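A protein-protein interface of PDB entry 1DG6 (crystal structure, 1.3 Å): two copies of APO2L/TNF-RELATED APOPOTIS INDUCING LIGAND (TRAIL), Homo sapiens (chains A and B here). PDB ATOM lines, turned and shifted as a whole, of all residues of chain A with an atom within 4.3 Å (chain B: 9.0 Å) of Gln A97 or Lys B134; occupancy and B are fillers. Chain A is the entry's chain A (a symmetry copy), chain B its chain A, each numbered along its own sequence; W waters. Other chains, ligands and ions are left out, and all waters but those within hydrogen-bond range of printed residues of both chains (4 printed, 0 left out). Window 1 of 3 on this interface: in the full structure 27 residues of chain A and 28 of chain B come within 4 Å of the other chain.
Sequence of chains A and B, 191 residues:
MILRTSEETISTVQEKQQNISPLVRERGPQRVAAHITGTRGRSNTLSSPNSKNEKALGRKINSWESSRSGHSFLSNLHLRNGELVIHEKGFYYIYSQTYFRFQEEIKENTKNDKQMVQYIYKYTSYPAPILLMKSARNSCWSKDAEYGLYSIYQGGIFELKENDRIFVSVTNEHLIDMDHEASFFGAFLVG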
ATOM      1  N   SER A  96      31.182  26.226   0.662  1.00  0.00           N
ATOM      2  CA  SER A  96      30.755  25.523  -0.544  1.00  0.00           C
ATOM      3  C   SER A  96      29.762  24.454  -0.182  1.00  0.00           C
ATOM      4  O   SER A  96      29.900  23.818   0.879  1.00  0.00           O
ATOM      5  CB  SER A  96      31.942  24.938  -1.302  1.00  0.00           C
ATOM      6  OG  SER A  96      31.490  24.268  -2.494  1.00  0.00           O
ATOM      7  N   GLN A  97      28.776  24.219  -1.084  1.00  0.00           N
ATOM      8  CA  GLN A  97      27.911  23.033  -1.005  1.00  0.00           C
ATOM      9  C   GLN A  97      28.122  22.260  -2.303  1.00  0.00           C
ATOM     10  O   GLN A  97      28.089  22.843  -3.387  1.00  0.00           O
ATOM     11  CB  GLN A  97      26.421  23.420  -0.834  1.00  0.00           C
ATOM     12  CG  GLN A  97      25.580  22.141  -0.630  1.00  0.00           C
ATOM     13  CD  GLN A  97      24.271  22.445   0.026  1.00  0.00           C
ATOM     14  OE1 GLN A  97      24.074  22.093   1.176  1.00  0.00           O
ATOM     15  NE2 GLN A  97      23.295  23.048  -0.640  1.00  0.00           N
ATOM     16  N   THR A  98      28.385  20.974  -2.163  1.00  0.00           N
ATOM     17  CA  THR A  98      28.558  20.129  -3.337  1.00  0.00           C
ATOM     18  C   THR A  98      27.638  18.932  -3.184  1.00  0.00           C
ATOM     19  O   THR A  98      27.727  18.204  -2.203  1.00  0.00           O
ATOM     20  CB  THR A  98      30.016  19.646  -3.491  1.00  0.00           C
ATOM     21  OG1 THR A  98      30.484  19.108  -2.263  1.00  0.00           O
ATOM     22  CG2 THR A  98      30.913  20.816  -3.896  1.00  0.00           C
ATOM     23  N   TYR A  99      26.741  18.754  -4.169  1.00  0.00           N
ATOM     24  CA  TYR A  99      25.742  17.665  -4.095  1.00  0.00           C
ATOM     25  C   TYR A  99      26.228  16.413  -4.800  1.00  0.00           C
ATOM     26  O   TYR A  99      26.306  16.412  -6.040  1.00  0.00           O
ATOM     27  CB  TYR A  99      24.465  18.142  -4.780  1.00  0.00           C
ATOM     28  CG  TYR A  99      23.240  17.281  -4.639  1.00  0.00           C
ATOM     29  CD1 TYR A  99      23.125  16.312  -3.655  1.00  0.00           C
ATOM     30  CD2 TYR A  99      22.149  17.436  -5.504  1.00  0.00           C
ATOM     31  CE1 TYR A  99      21.982  15.536  -3.531  1.00  0.00           C
ATOM     32  CE2 TYR A  99      21.011  16.657  -5.405  1.00  0.00           C
ATOM     33  CZ  TYR A  99      20.932  15.703  -4.406  1.00  0.00           C
ATOM     34  OH  TYR A  99      19.806  14.923  -4.210  1.00  0.00           O
ATOM     35  N   GLN A 118      34.825  16.925   0.020  1.00  0.00           N
ATOM     36  CA  GLN A 118      34.940  18.281  -0.550  1.00  0.00           C
ATOM     37  C   GLN A 118      36.136  18.957   0.096  1.00  0.00           C
ATOM     38  O   GLN A 118      36.256  18.965   1.335  1.00  0.00           O
ATOM     39  CB  GLN A 118      33.633  19.058  -0.249  1.00  0.00           C
ATOM     40  CG  GLN A 118      33.598  20.436  -0.930  1.00  0.00           C
ATOM     41  CD  GLN A 118      32.734  21.431  -0.168  1.00  0.00           C
ATOM     42  OE1 GLN A 118      33.234  22.321   0.536  1.00  0.00           O
ATOM     43  NE2 GLN A 118      31.389  21.252  -0.256  1.00  0.00           N
ATOM     44  N   SER A 151      24.487  15.745   0.048  1.00  0.00           N
ATOM     45  CA  SER A 151      24.886  17.163  -0.064  1.00  0.00           C
ATOM     46  C   SER A 151      25.896  17.435   1.064  1.00  0.00           C
ATOM     47  O   SER A 151      25.575  17.168   2.250  1.00  0.00           O
ATOM     48  CB  SER A 151      23.686  18.087   0.166  1.00  0.00           C
ATOM     49  OG  SER A 151      22.744  17.904  -0.881  1.00  0.00           O
ATOM     50  N   ILE A 152      27.035  18.008   0.703  1.00  0.00           N
ATOM     51  CA  ILE A 152      28.077  18.387   1.666  1.00  0.00           C
ATOM     52  C   ILE A 152      28.252  19.894   1.672  1.00  0.00           C
ATOM     53  O   ILE A 152      28.606  20.463   0.619  1.00  0.00           O
ATOM     54  CB  ILE A 152      29.413  17.696   1.307  1.00  0.00           C
ATOM     55  CG1 ILE A 152      29.234  16.163   1.446  1.00  0.00           C
ATOM     56  CG2 ILE A 152      30.501  18.257   2.196  1.00  0.00           C
ATOM     57  CD1 ILE A 152      30.546  15.423   1.134  1.00  0.00           C
ATOM     58  N   TYR A 153      28.029  20.506   2.830  1.00  0.00           N
ATOM     59  CA  TYR A 153      28.235  21.925   3.053  1.00  0.00           C
ATOM     60  C   TYR A 153      29.391  22.027   4.072  1.00  0.00           C
ATOM     61  O   TYR A 153      29.283  21.426   5.144  1.00  0.00           O
ATOM     62  CB  TYR A 153      26.952  22.641   3.574  1.00  0.00           C
ATOM     63  CG  TYR A 153      27.222  24.107   3.897  1.00  0.00           C
ATOM     64  CD1 TYR A 153      27.791  24.530   5.105  1.00  0.00           C
ATOM     65  CD2 TYR A 153      26.935  25.120   2.968  1.00  0.00           C
ATOM     66  CE1 TYR A 153      28.071  25.832   5.424  1.00  0.00           C
ATOM     67  CE2 TYR A 153      27.202  26.455   3.266  1.00  0.00           C
ATOM     68  CZ  TYR A 153      27.756  26.794   4.479  1.00  0.00           C
ATOM     69  OH  TYR A 153      28.040  28.111   4.776  1.00  0.00           O
ATOM     70  N   GLU A 181      20.911  25.283  -7.616  1.00  0.00           N
ATOM     71  CA  GLU A 181      20.451  25.449  -6.239  1.00  0.00           C
ATOM     72  C   GLU A 181      21.146  24.419  -5.313  1.00  0.00           C
ATOM     73  O   GLU A 181      21.078  24.536  -4.082  1.00  0.00           O
ATOM     74  CB  GLU A 181      18.938  25.230  -6.099  1.00  0.00           C
ATOM     75  CG  GLU A 181      18.109  26.040  -7.077  1.00  0.00           C
ATOM     76  CD  GLU A 181      17.734  25.244  -8.320  1.00  0.00           C
ATOM     77  OE1 GLU A 181      18.574  24.424  -8.806  1.00  0.00           O
ATOM     78  OE2 GLU A 181      16.605  25.352  -8.845  1.00  0.00           O
ATOM     79  N   ALA A 182      21.788  23.401  -5.916  1.00  0.00           N
ATOM     80  CA  ALA A 182      22.326  22.297  -5.101  1.00  0.00           C
ATOM     81  C   ALA A 182      23.830  22.423  -4.842  1.00  0.00           C
ATOM     82  O   ALA A 182      24.288  21.969  -3.783  1.00  0.00           O
ATOM     83  CB  ALA A 182      22.026  20.976  -5.769  1.00  0.00           C
ATOM     84  N   SER A 183      24.554  22.964  -5.810  1.00  0.00           N
ATOM     85  CA  SER A 183      26.019  23.018  -5.711  1.00  0.00           C
ATOM     86  C   SER A 183      26.436  24.471  -5.952  1.00  0.00           C
ATOM     87  O   SER A 183      26.004  25.086  -6.951  1.00  0.00           O
ATOM     88  CB  SER A 183      26.739  22.107  -6.689  1.00  0.00           C
ATOM     89  OG  SER A 183      26.462  20.718  -6.357  1.00  0.00           O
ATOM     90  N   PHE A 184      27.277  25.000  -5.068  1.00  0.00           N
ATOM     91  CA  PHE A 184      27.656  26.412  -5.123  1.00  0.00           C
ATOM     92  C   PHE A 184      28.854  26.676  -4.247  1.00  0.00           C
ATOM     93  O   PHE A 184      29.284  25.817  -3.447  1.00  0.00           O
ATOM     94  CB  PHE A 184      26.453  27.307  -4.748  1.00  0.00           C
ATOM     95  CG  PHE A 184      25.742  26.933  -3.439  1.00  0.00           C
ATOM     96  CD1 PHE A 184      26.307  27.188  -2.218  1.00  0.00           C
ATOM     97  CD2 PHE A 184      24.488  26.332  -3.456  1.00  0.00           C
ATOM     98  CE1 PHE A 184      25.651  26.958  -1.000  1.00  0.00           C
ATOM     99  CE2 PHE A 184      23.839  26.066  -2.283  1.00  0.00           C
ATOM    100  CZ  PHE A 184      24.364  26.358  -1.054  1.00  0.00           C
ATOM    101  N   LEU B  57       8.315  22.943  -3.830  1.00  0.00           N
ATOM    102  CA  LEU B  57       8.447  21.579  -3.385  1.00  0.00           C
ATOM    103  C   LEU B  57       8.407  21.477  -1.866  1.00  0.00           C
ATOM    104  O   LEU B  57       8.608  22.451  -1.127  1.00  0.00           O
ATOM    105  CB  LEU B  57       9.771  21.011  -3.889  1.00  0.00           C
ATOM    106  CG  LEU B  57       9.889  20.975  -5.417  1.00  0.00           C
ATOM    107  CD1 LEU B  57      11.316  20.684  -5.841  1.00  0.00           C
ATOM    108  CD2 LEU B  57       8.961  19.910  -5.986  1.00  0.00           C
ATOM    109  N   TYR B  93      23.429  36.533   3.881  1.00  0.00           N
ATOM    110  CA  TYR B  93      23.705  35.121   4.106  1.00  0.00           C
ATOM    111  C   TYR B  93      22.479  34.522   4.784  1.00  0.00           C
ATOM    112  O   TYR B  93      22.054  35.005   5.852  1.00  0.00           O
ATOM    113  CB  TYR B  93      24.988  34.989   4.976  1.00  0.00           C
ATOM    114  CG  TYR B  93      25.279  33.514   5.192  1.00  0.00           C
ATOM    115  CD1 TYR B  93      26.007  32.764   4.283  1.00  0.00           C
ATOM    116  CD2 TYR B  93      24.827  32.850   6.350  1.00  0.00           C
ATOM    117  CE1 TYR B  93      26.270  31.417   4.490  1.00  0.00           C
ATOM    118  CE2 TYR B  93      25.099  31.496   6.569  1.00  0.00           C
ATOM    119  CZ  TYR B  93      25.832  30.778   5.625  1.00  0.00           C
ATOM    120  OH  TYR B  93      26.015  29.440   5.890  1.00  0.00           O
ATOM    121  N   SER B  96      19.642  27.516   7.116  1.00  0.00           N
ATOM    122  CA  SER B  96      18.680  26.759   7.912  1.00  0.00           C
ATOM    123  C   SER B  96      19.288  25.448   8.327  1.00  0.00           C
ATOM    124  O   SER B  96      20.043  24.842   7.544  1.00  0.00           O
ATOM    125  CB  SER B  96      17.371  26.546   7.157  1.00  0.00           C
ATOM    126  OG  SER B  96      16.440  25.813   7.974  1.00  0.00           O
ATOM    127  N   MET B 116      15.296  12.907   2.412  1.00  0.00           N
ATOM    128  CA  MET B 116      15.125  14.037   3.313  1.00  0.00           C
ATOM    129  C   MET B 116      15.749  15.253   2.642  1.00  0.00           C
ATOM    130  O   MET B 116      16.966  15.247   2.466  1.00  0.00           O
ATOM    131  CB  MET B 116      15.821  13.699   4.630  1.00  0.00           C
ATOM    132  CG  MET B 116      15.065  12.565   5.369  1.00  0.00           C
ATOM    133  SD  MET B 116      16.116  11.774   6.618  1.00  0.00           S
ATOM    134  CE  MET B 116      17.221  10.799   5.594  1.00  0.00           C
ATOM    135  N   VAL B 117      14.925  16.211   2.243  1.00  0.00           N
ATOM    136  CA  VAL B 117      15.404  17.370   1.488  1.00  0.00           C
ATOM    137  C   VAL B 117      14.939  18.660   2.189  1.00  0.00           C
ATOM    138  O   VAL B 117      13.782  18.758   2.617  1.00  0.00           O
ATOM    139  CB  VAL B 117      14.891  17.355   0.042  1.00  0.00           C
ATOM    140  CG1 VAL B 117      15.580  18.425  -0.805  1.00  0.00           C
ATOM    141  CG2 VAL B 117      15.062  15.949  -0.585  1.00  0.00           C
ATOM    142  N   GLN B 118      15.885  19.600   2.277  1.00  0.00           N
ATOM    143  CA  GLN B 118      15.555  20.952   2.767  1.00  0.00           C
ATOM    144  C   GLN B 118      15.666  21.912   1.595  1.00  0.00           C
ATOM    145  O   GLN B 118      16.688  21.915   0.886  1.00  0.00           O
ATOM    146  CB  GLN B 118      16.551  21.330   3.891  1.00  0.00           C
ATOM    147  CG  GLN B 118      16.198  22.665   4.568  1.00  0.00           C
ATOM    148  CD  GLN B 118      17.424  23.360   5.142  1.00  0.00           C
ATOM    149  OE1 GLN B 118      17.944  24.332   4.575  1.00  0.00           O
ATOM    150  NE2 GLN B 118      17.947  22.820   6.275  1.00  0.00           N
ATOM    151  N   TYR B 119      14.620  22.720   1.420  1.00  0.00           N
ATOM    152  CA  TYR B 119      14.551  23.732   0.398  1.00  0.00           C
ATOM    153  C   TYR B 119      14.458  25.146   1.033  1.00  0.00           C
ATOM    154  O   TYR B 119      13.703  25.271   2.021  1.00  0.00           O
ATOM    155  CB  TYR B 119      13.269  23.543  -0.426  1.00  0.00           C
ATOM    156  CG  TYR B 119      13.117  22.201  -1.114  1.00  0.00           C
ATOM    157  CD1 TYR B 119      13.740  21.908  -2.307  1.00  0.00           C
ATOM    158  CD2 TYR B 119      12.308  21.221  -0.542  1.00  0.00           C
ATOM    159  CE1 TYR B 119      13.609  20.699  -2.972  1.00  0.00           C
ATOM    160  CE2 TYR B 119      12.163  20.020  -1.178  1.00  0.00           C
ATOM    161  CZ  TYR B 119      12.798  19.740  -2.375  1.00  0.00           C
ATOM    162  OH  TYR B 119      12.609  18.492  -2.955  1.00  0.00           O
ATOM    163  N   ILE B 120      15.187  26.123   0.490  1.00  0.00           N
ATOM    164  CA  ILE B 120      15.044  27.507   0.933  1.00  0.00           C
ATOM    165  C   ILE B 120      14.592  28.296  -0.290  1.00  0.00           C
ATOM    166  O   ILE B 120      15.257  28.269  -1.341  1.00  0.00           O
ATOM    167  CB  ILE B 120      16.351  28.060   1.536  1.00  0.00           C
ATOM    168  CG1 ILE B 120      16.733  27.239   2.772  1.00  0.00           C
ATOM    169  CG2 ILE B 120      16.171  29.539   1.847  1.00  0.00           C
ATOM    170  CD1 ILE B 120      18.111  27.552   3.383  1.00  0.00           C
ATOM    171  N   TYR B 121      13.423  28.882  -0.139  1.00  0.00           N
ATOM    172  CA  TYR B 121      12.713  29.570  -1.193  1.00  0.00           C
ATOM    173  C   TYR B 121      12.602  31.081  -0.921  1.00  0.00           C
ATOM    174  O   TYR B 121      12.621  31.527   0.235  1.00  0.00           O
ATOM    175  CB  TYR B 121      11.255  29.051  -1.257  1.00  0.00           C
ATOM    176  CG  TYR B 121      11.108  27.794  -2.097  1.00  0.00           C
ATOM    177  CD1 TYR B 121      11.040  27.873  -3.481  1.00  0.00           C
ATOM    178  CD2 TYR B 121      11.056  26.513  -1.509  1.00  0.00           C
ATOM    179  CE1 TYR B 121      10.909  26.730  -4.277  1.00  0.00           C
ATOM    180  CE2 TYR B 121      10.943  25.364  -2.295  1.00  0.00           C
ATOM    181  CZ  TYR B 121      10.854  25.476  -3.668  1.00  0.00           C
ATOM    182  OH  TYR B 121      10.761  24.312  -4.450  1.00  0.00           O
ATOM    183  N   LEU B 131      13.323  28.900  -5.911  1.00  0.00           N
ATOM    184  CA  LEU B 131      14.216  28.102  -5.060  1.00  0.00           C
ATOM    185  C   LEU B 131      15.601  28.713  -5.060  1.00  0.00           C
ATOM    186  O   LEU B 131      16.183  28.962  -6.140  1.00  0.00           O
ATOM    187  CB  LEU B 131      14.256  26.662  -5.660  1.00  0.00           C
ATOM    188  CG  LEU B 131      15.146  25.673  -4.841  1.00  0.00           C
ATOM    189  CD1 LEU B 131      14.648  25.540  -3.402  1.00  0.00           C
ATOM    190  CD2 LEU B 131      15.118  24.316  -5.525  1.00  0.00           C
ATOM    191  N   LEU B 132      16.126  28.954  -3.860  1.00  0.00           N
ATOM    192  CA  LEU B 132      17.496  29.444  -3.724  1.00  0.00           C
ATOM    193  C   LEU B 132      18.497  28.302  -3.505  1.00  0.00           C
ATOM    194  O   LEU B 132      19.566  28.300  -4.127  1.00  0.00           O
ATOM    195  CB  LEU B 132      17.619  30.403  -2.551  1.00  0.00           C
ATOM    196  CG  LEU B 132      16.697  31.611  -2.618  1.00  0.00           C
ATOM    197  CD1 LEU B 132      17.022  32.517  -1.419  1.00  0.00           C
ATOM    198  CD2 LEU B 132      16.837  32.340  -3.925  1.00  0.00           C
ATOM    199  N   MET B 133      18.166  27.374  -2.601  1.00  0.00           N
ATOM    200  CA  MET B 133      19.121  26.332  -2.164  1.00  0.00           C
ATOM    201  C   MET B 133      18.364  25.057  -1.833  1.00  0.00           C
ATOM    202  O   MET B 133      17.252  25.089  -1.272  1.00  0.00           O
ATOM    203  CB  MET B 133      19.845  26.737  -0.866  1.00  0.00           C
ATOM    204  CG  MET B 133      20.797  27.920  -1.060  1.00  0.00           C
ATOM    205  SD  MET B 133      21.508  28.454   0.530  1.00  0.00           S
ATOM    206  CE  MET B 133      20.233  29.533   1.157  1.00  0.00           C
ATOM    207  N   LYS B 134      18.989  23.936  -2.189  1.00  0.00           N
ATOM    208  CA  LYS B 134      18.432  22.642  -1.741  1.00  0.00           C
ATOM    209  C   LYS B 134      19.555  21.753  -1.236  1.00  0.00           C
ATOM    210  O   LYS B 134      20.657  21.761  -1.813  1.00  0.00           O
ATOM    211  CB  LYS B 134      17.673  21.964  -2.859  1.00  0.00           C
ATOM    212  CG  LYS B 134      18.422  21.453  -4.036  1.00  0.00           C
ATOM    213  CD  LYS B 134      17.470  20.594  -4.908  1.00  0.00           C
ATOM    214  CE  LYS B 134      18.127  19.227  -5.108  1.00  0.00           C
ATOM    215  NZ  LYS B 134      19.410  19.352  -5.871  1.00  0.00           N
ATOM    216  N   SER B 135      19.274  20.944  -0.200  1.00  0.00           N
ATOM    217  CA  SER B 135      20.237  20.028   0.403  1.00  0.00           C
ATOM    218  C   SER B 135      19.523  18.722   0.746  1.00  0.00           C
ATOM    219  O   SER B 135      18.429  18.773   1.285  1.00  0.00           O
ATOM    220  CB  SER B 135      20.870  20.690   1.643  1.00  0.00           C
ATOM    221  OG  SER B 135      21.792  19.776   2.244  1.00  0.00           O
ATOM    222  N   ALA B 136      20.112  17.587   0.366  1.00  0.00           N
ATOM    223  CA  ALA B 136      19.428  16.297   0.475  1.00  0.00           C
ATOM    224  C   ALA B 136      20.288  15.209   1.108  1.00  0.00           C
ATOM    225  O   ALA B 136      21.530  15.199   1.013  1.00  0.00           O
ATOM    226  CB  ALA B 136      18.986  15.797  -0.914  1.00  0.00           C
ATOM    227  N   ARG B 137      19.578  14.291   1.765  1.00  0.00           N
ATOM    228  CA  ARG B 137      20.146  13.054   2.293  1.00  0.00           C
ATOM    229  C   ARG B 137      19.192  11.912   2.007  1.00  0.00           C
ATOM    230  O   ARG B 137      17.975  12.124   1.981  1.00  0.00           O
ATOM    231  CB  ARG B 137      20.401  13.100   3.796  1.00  0.00           C
ATOM    232  CG  ARG B 137      21.619  13.930   4.194  1.00  0.00           C
ATOM    233  CD  ARG B 137      22.935  13.308   3.784  1.00  0.00           C
ATOM    234  NE  ARG B 137      23.140  12.013   4.423  1.00  0.00           N
ATOM    235  CZ  ARG B 137      23.011  10.788   3.939  1.00  0.00           C
ATOM    236  NH1 ARG B 137      22.651  10.594   2.698  1.00  0.00           N
ATOM    237  NH2 ARG B 137      23.247   9.731   4.721  1.00  0.00           N
ATOM    238  N   ILE B 152      20.294  18.477   8.728  1.00  0.00           N
ATOM    239  CA  ILE B 152      20.705  19.099   7.462  1.00  0.00           C
ATOM    240  C   ILE B 152      20.871  20.595   7.652  1.00  0.00           C
ATOM    241  O   ILE B 152      19.881  21.271   8.003  1.00  0.00           O
ATOM    242  CB  ILE B 152      19.658  18.813   6.362  1.00  0.00           C
ATOM    243  CG1 ILE B 152      19.616  17.287   6.097  1.00  0.00           C
ATOM    244  CG2 ILE B 152      20.013  19.626   5.136  1.00  0.00           C
ATOM    245  CD1 ILE B 152      18.613  16.946   4.983  1.00  0.00           C
ATOM    246  N   TYR B 153      22.081  21.087   7.406  1.00  0.00           N
ATOM    247  CA  TYR B 153      22.406  22.501   7.443  1.00  0.00           C
ATOM    248  C   TYR B 153      22.768  22.887   5.992  1.00  0.00           C
ATOM    249  O   TYR B 153      23.654  22.248   5.418  1.00  0.00           O
ATOM    250  CB  TYR B 153      23.573  22.821   8.425  1.00  0.00           C
ATOM    251  CG  TYR B 153      23.964  24.294   8.370  1.00  0.00           C
ATOM    252  CD1 TYR B 153      24.817  24.821   7.391  1.00  0.00           C
ATOM    253  CD2 TYR B 153      23.454  25.216   9.297  1.00  0.00           C
ATOM    254  CE1 TYR B 153      25.172  26.140   7.291  1.00  0.00           C
ATOM    255  CE2 TYR B 153      23.802  26.563   9.227  1.00  0.00           C
ATOM    256  CZ  TYR B 153      24.653  27.006   8.239  1.00  0.00           C
ATOM    257  OH  TYR B 153      24.989  28.340   8.151  1.00  0.00           O
ATOM    258  N   GLN B 154      22.315  24.065   5.538  1.00  0.00           N
ATOM    259  CA  GLN B 154      22.915  24.713   4.374  1.00  0.00           C
ATOM    260  C   GLN B 154      22.768  26.208   4.530  1.00  0.00           C
ATOM    261  O   GLN B 154      21.935  26.703   5.317  1.00  0.00           O
ATOM    262  CB  GLN B 154      22.274  24.298   3.053  1.00  0.00           C
ATOM    263  CG  GLN B 154      20.839  24.821   2.899  1.00  0.00           C
ATOM    264  CD  GLN B 154      20.118  24.230   1.663  1.00  0.00           C
ATOM    265  OE1 GLN B 154      20.751  23.882   0.686  1.00  0.00           O
ATOM    266  NE2 GLN B 154      18.798  24.112   1.815  1.00  0.00           N
ATOM    267  N   GLY B 155      23.578  26.943   3.773  1.00  0.00           N
ATOM    268  CA  GLY B 155      23.378  28.392   3.700  1.00  0.00           C
ATOM    269  C   GLY B 155      24.120  28.971   2.498  1.00  0.00           C
ATOM    270  O   GLY B 155      24.927  28.265   1.861  1.00  0.00           O
ATOM    271  N   GLY B 156      23.891  30.232   2.224  1.00  0.00           N
ATOM    272  CA  GLY B 156      24.554  30.878   1.076  1.00  0.00           C
ATOM    273  C   GLY B 156      24.127  32.342   0.983  1.00  0.00           C
ATOM    274  O   GLY B 156      23.208  32.762   1.697  1.00  0.00           O
ATOM    275  N   PHE B 158      22.634  35.606  -0.972  1.00  0.00           N
ATOM    276  CA  PHE B 158      21.704  35.981  -2.036  1.00  0.00           C
ATOM    277  C   PHE B 158      21.352  37.449  -1.957  1.00  0.00           C
ATOM    278  O   PHE B 158      21.209  38.022  -0.855  1.00  0.00           O
ATOM    279  CB  PHE B 158      20.398  35.121  -1.938  1.00  0.00           C
ATOM    280  CG  PHE B 158      20.704  33.651  -2.205  1.00  0.00           C
ATOM    281  CD1 PHE B 158      21.162  32.841  -1.150  1.00  0.00           C
ATOM    282  CD2 PHE B 158      20.625  33.123  -3.487  1.00  0.00           C
ATOM    283  CE1 PHE B 158      21.573  31.542  -1.403  1.00  0.00           C
ATOM    284  CE2 PHE B 158      20.982  31.791  -3.736  1.00  0.00           C
ATOM    285  CZ  PHE B 158      21.486  31.012  -2.698  1.00  0.00           C
ATOM    286  N   SER B 169      11.224  24.864   3.312  1.00  0.00           N
ATOM    287  CA  SER B 169      10.308  23.735   3.148  1.00  0.00           C
ATOM    288  C   SER B 169      11.099  22.444   3.194  1.00  0.00           C
ATOM    289  O   SER B 169      12.311  22.426   2.921  1.00  0.00           O
ATOM    290  CB  SER B 169       9.490  23.905   1.875  1.00  0.00           C
ATOM    291  OG  SER B 169      10.259  23.640   0.737  1.00  0.00           O
HETATM  292  O   HOH W   1      15.659  28.495  -8.785  1.00  0.00           O
HETATM  293  O   HOH W   2      22.817  20.189  -2.266  1.00  0.00           O
HETATM  294  O   HOH W   3      26.438  21.097   6.878  1.00  0.00           O
HETATM  295  O   HOH W   4      24.108  20.606   3.394  1.00  0.00           O
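The side-chain hydroxyl (OH) of Tyr A153 is in hydrogen-bond range of the side-chain hydroxyl (OH) of Tyr B93. The side-chain amide nitrogen (NE2) of Gln A97 sits at hydrogen-bond distance from the backbone carbonyl oxygen (O) of Lys B134, 3.2 Å away. O of Glu A181 sits at hydrogen-bond distance from N of Lys B134, 2.9 Å away. The side-chain hydroxyl (OG) of Ser B135 lies within hydrogen-bond range of the side-chain amide oxygen (OE1) of Gln A97, 3.4 Å away. The backbone NH (N) of Ala B136 lies within hydrogen-bond range of the side-chain hydroxyl (OG) of Ser A151, 2.9 Å away. The side-chain amide nitrogen (NE2) of Gln A97 sits at hydrogen-bond distance from the side-chain amide oxygen (OE1) of Gln B154, at 3.0 Å.
O of Ile B120 sits at hydrogen-bond distance from N of Leu B132. The side-chain sulfur (SD) of Met B133 lies within hydrogen-bond range of the backbone NH (N) of Gly B156, 3.4 Å away. The side-chain amide oxygen (OE1) of Gln B154 sits close to the backbone NH (N) of Ser B135. The side-chain amide nitrogen (NE2) of Gln A97 sits close to the backbone carbonyl oxygen (O) of Ala A182 (3.5 Å). The backbone NH (N) of Phe A184 sits at hydrogen-bond distance from the backbone carbonyl oxygen (O) of Gln A97 (2.9 Å). OG of Ser A183 sits at hydrogen-bond distance from N of Tyr A99 (3.0 Å).
Among the printed residues, pairs that only touch across the chains: Tyr A99 with Lys B134 (3.2 Å), Tyr A99 with Ala B136 (3.5 Å), Ser A151 with Ser B135 (3.3 Å), Tyr A153 with Tyr B153 (3.5 Å), Tyr A153 with Gly B155 (3.2 Å), Glu A181 with Leu B131 (3.6 Å), Glu A181 with Leu B132 (3.7 Å), Glu A181 with Met B133 (3.3 Å), Ala A182 with Lys B134 (3.1 Å), Phe A184 with Met B133 (3.8 Å) and Phe A184 with Gly B155 (3.2 Å).
Of the printed residues of chain B, Gln A97 touches Lys B134, Ser B135 and Gln B154. No residue of chain B comes within 4 Å of Ser A96. No residue of chain B comes within 4 Å of Thr A98. No residue of chain B comes within 4 Å of Ser A183. Phe A184 touches just these residues of chain B: Met B133 and Gly B155. Printed residues of chain A within 4 Å of Ser B135: Gln A97 (3.4 Å) and Ser A151 (3.3 Å). Printed residues of chain A within 4 Å of Met B133: Glu A181 (3.3 Å) and Phe A184 (3.8 Å). Of the printed residues of chain A, Ala B136 touches Tyr A99 and Ser A151. Of the printed residues of chain A, Leu B131 touches Glu A181 (3.6 Å).
Of the 23 printed residues of chain B, 10 touch a printed residue of chain A. Hydrophobic or aromatic side chains of chain B within 4 Å of the printed part of chain A: Tyr B93, Leu B131, Met B133, Ala B136 and Tyr B153. Along chain A the printed residues that touch a printed residue of chain B span positions 97 to 184. Among the printed residues, 17 pairs touch across the chains.
Tyr B153 touches its own counterpart, Tyr A153. Positions printed for both chains: 96, 118, 152 and 153.
Water W4 lies within hydrogen-bond range of O of Tyr B153 (2.6 Å), OE1 of Gln A97 (2.7 Å) and OG of Ser B135 (2.7 Å). Water W2 lies within hydrogen-bond range of the side-chain hydroxyl (OG) of Ser A151 (2.7 Å), the backbone carbonyl oxygen (O) of Lys B134 (2.7 Å), the backbone carbonyl oxygen (O) of Ala A182 (2.8 Å) and the side-chain amide nitrogen (NE2) of Gln A97 (3.3 Å). Water W1 bridges O of Leu B131 (2.7 Å) and OE2 of Glu A181 (3.3 Å). Water W3 lies within hydrogen-bond range of the backbone carbonyl oxygen of Tyr A153 (3.3 Å) and the backbone carbonyl oxygen of Tyr B153 (3.3 Å).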
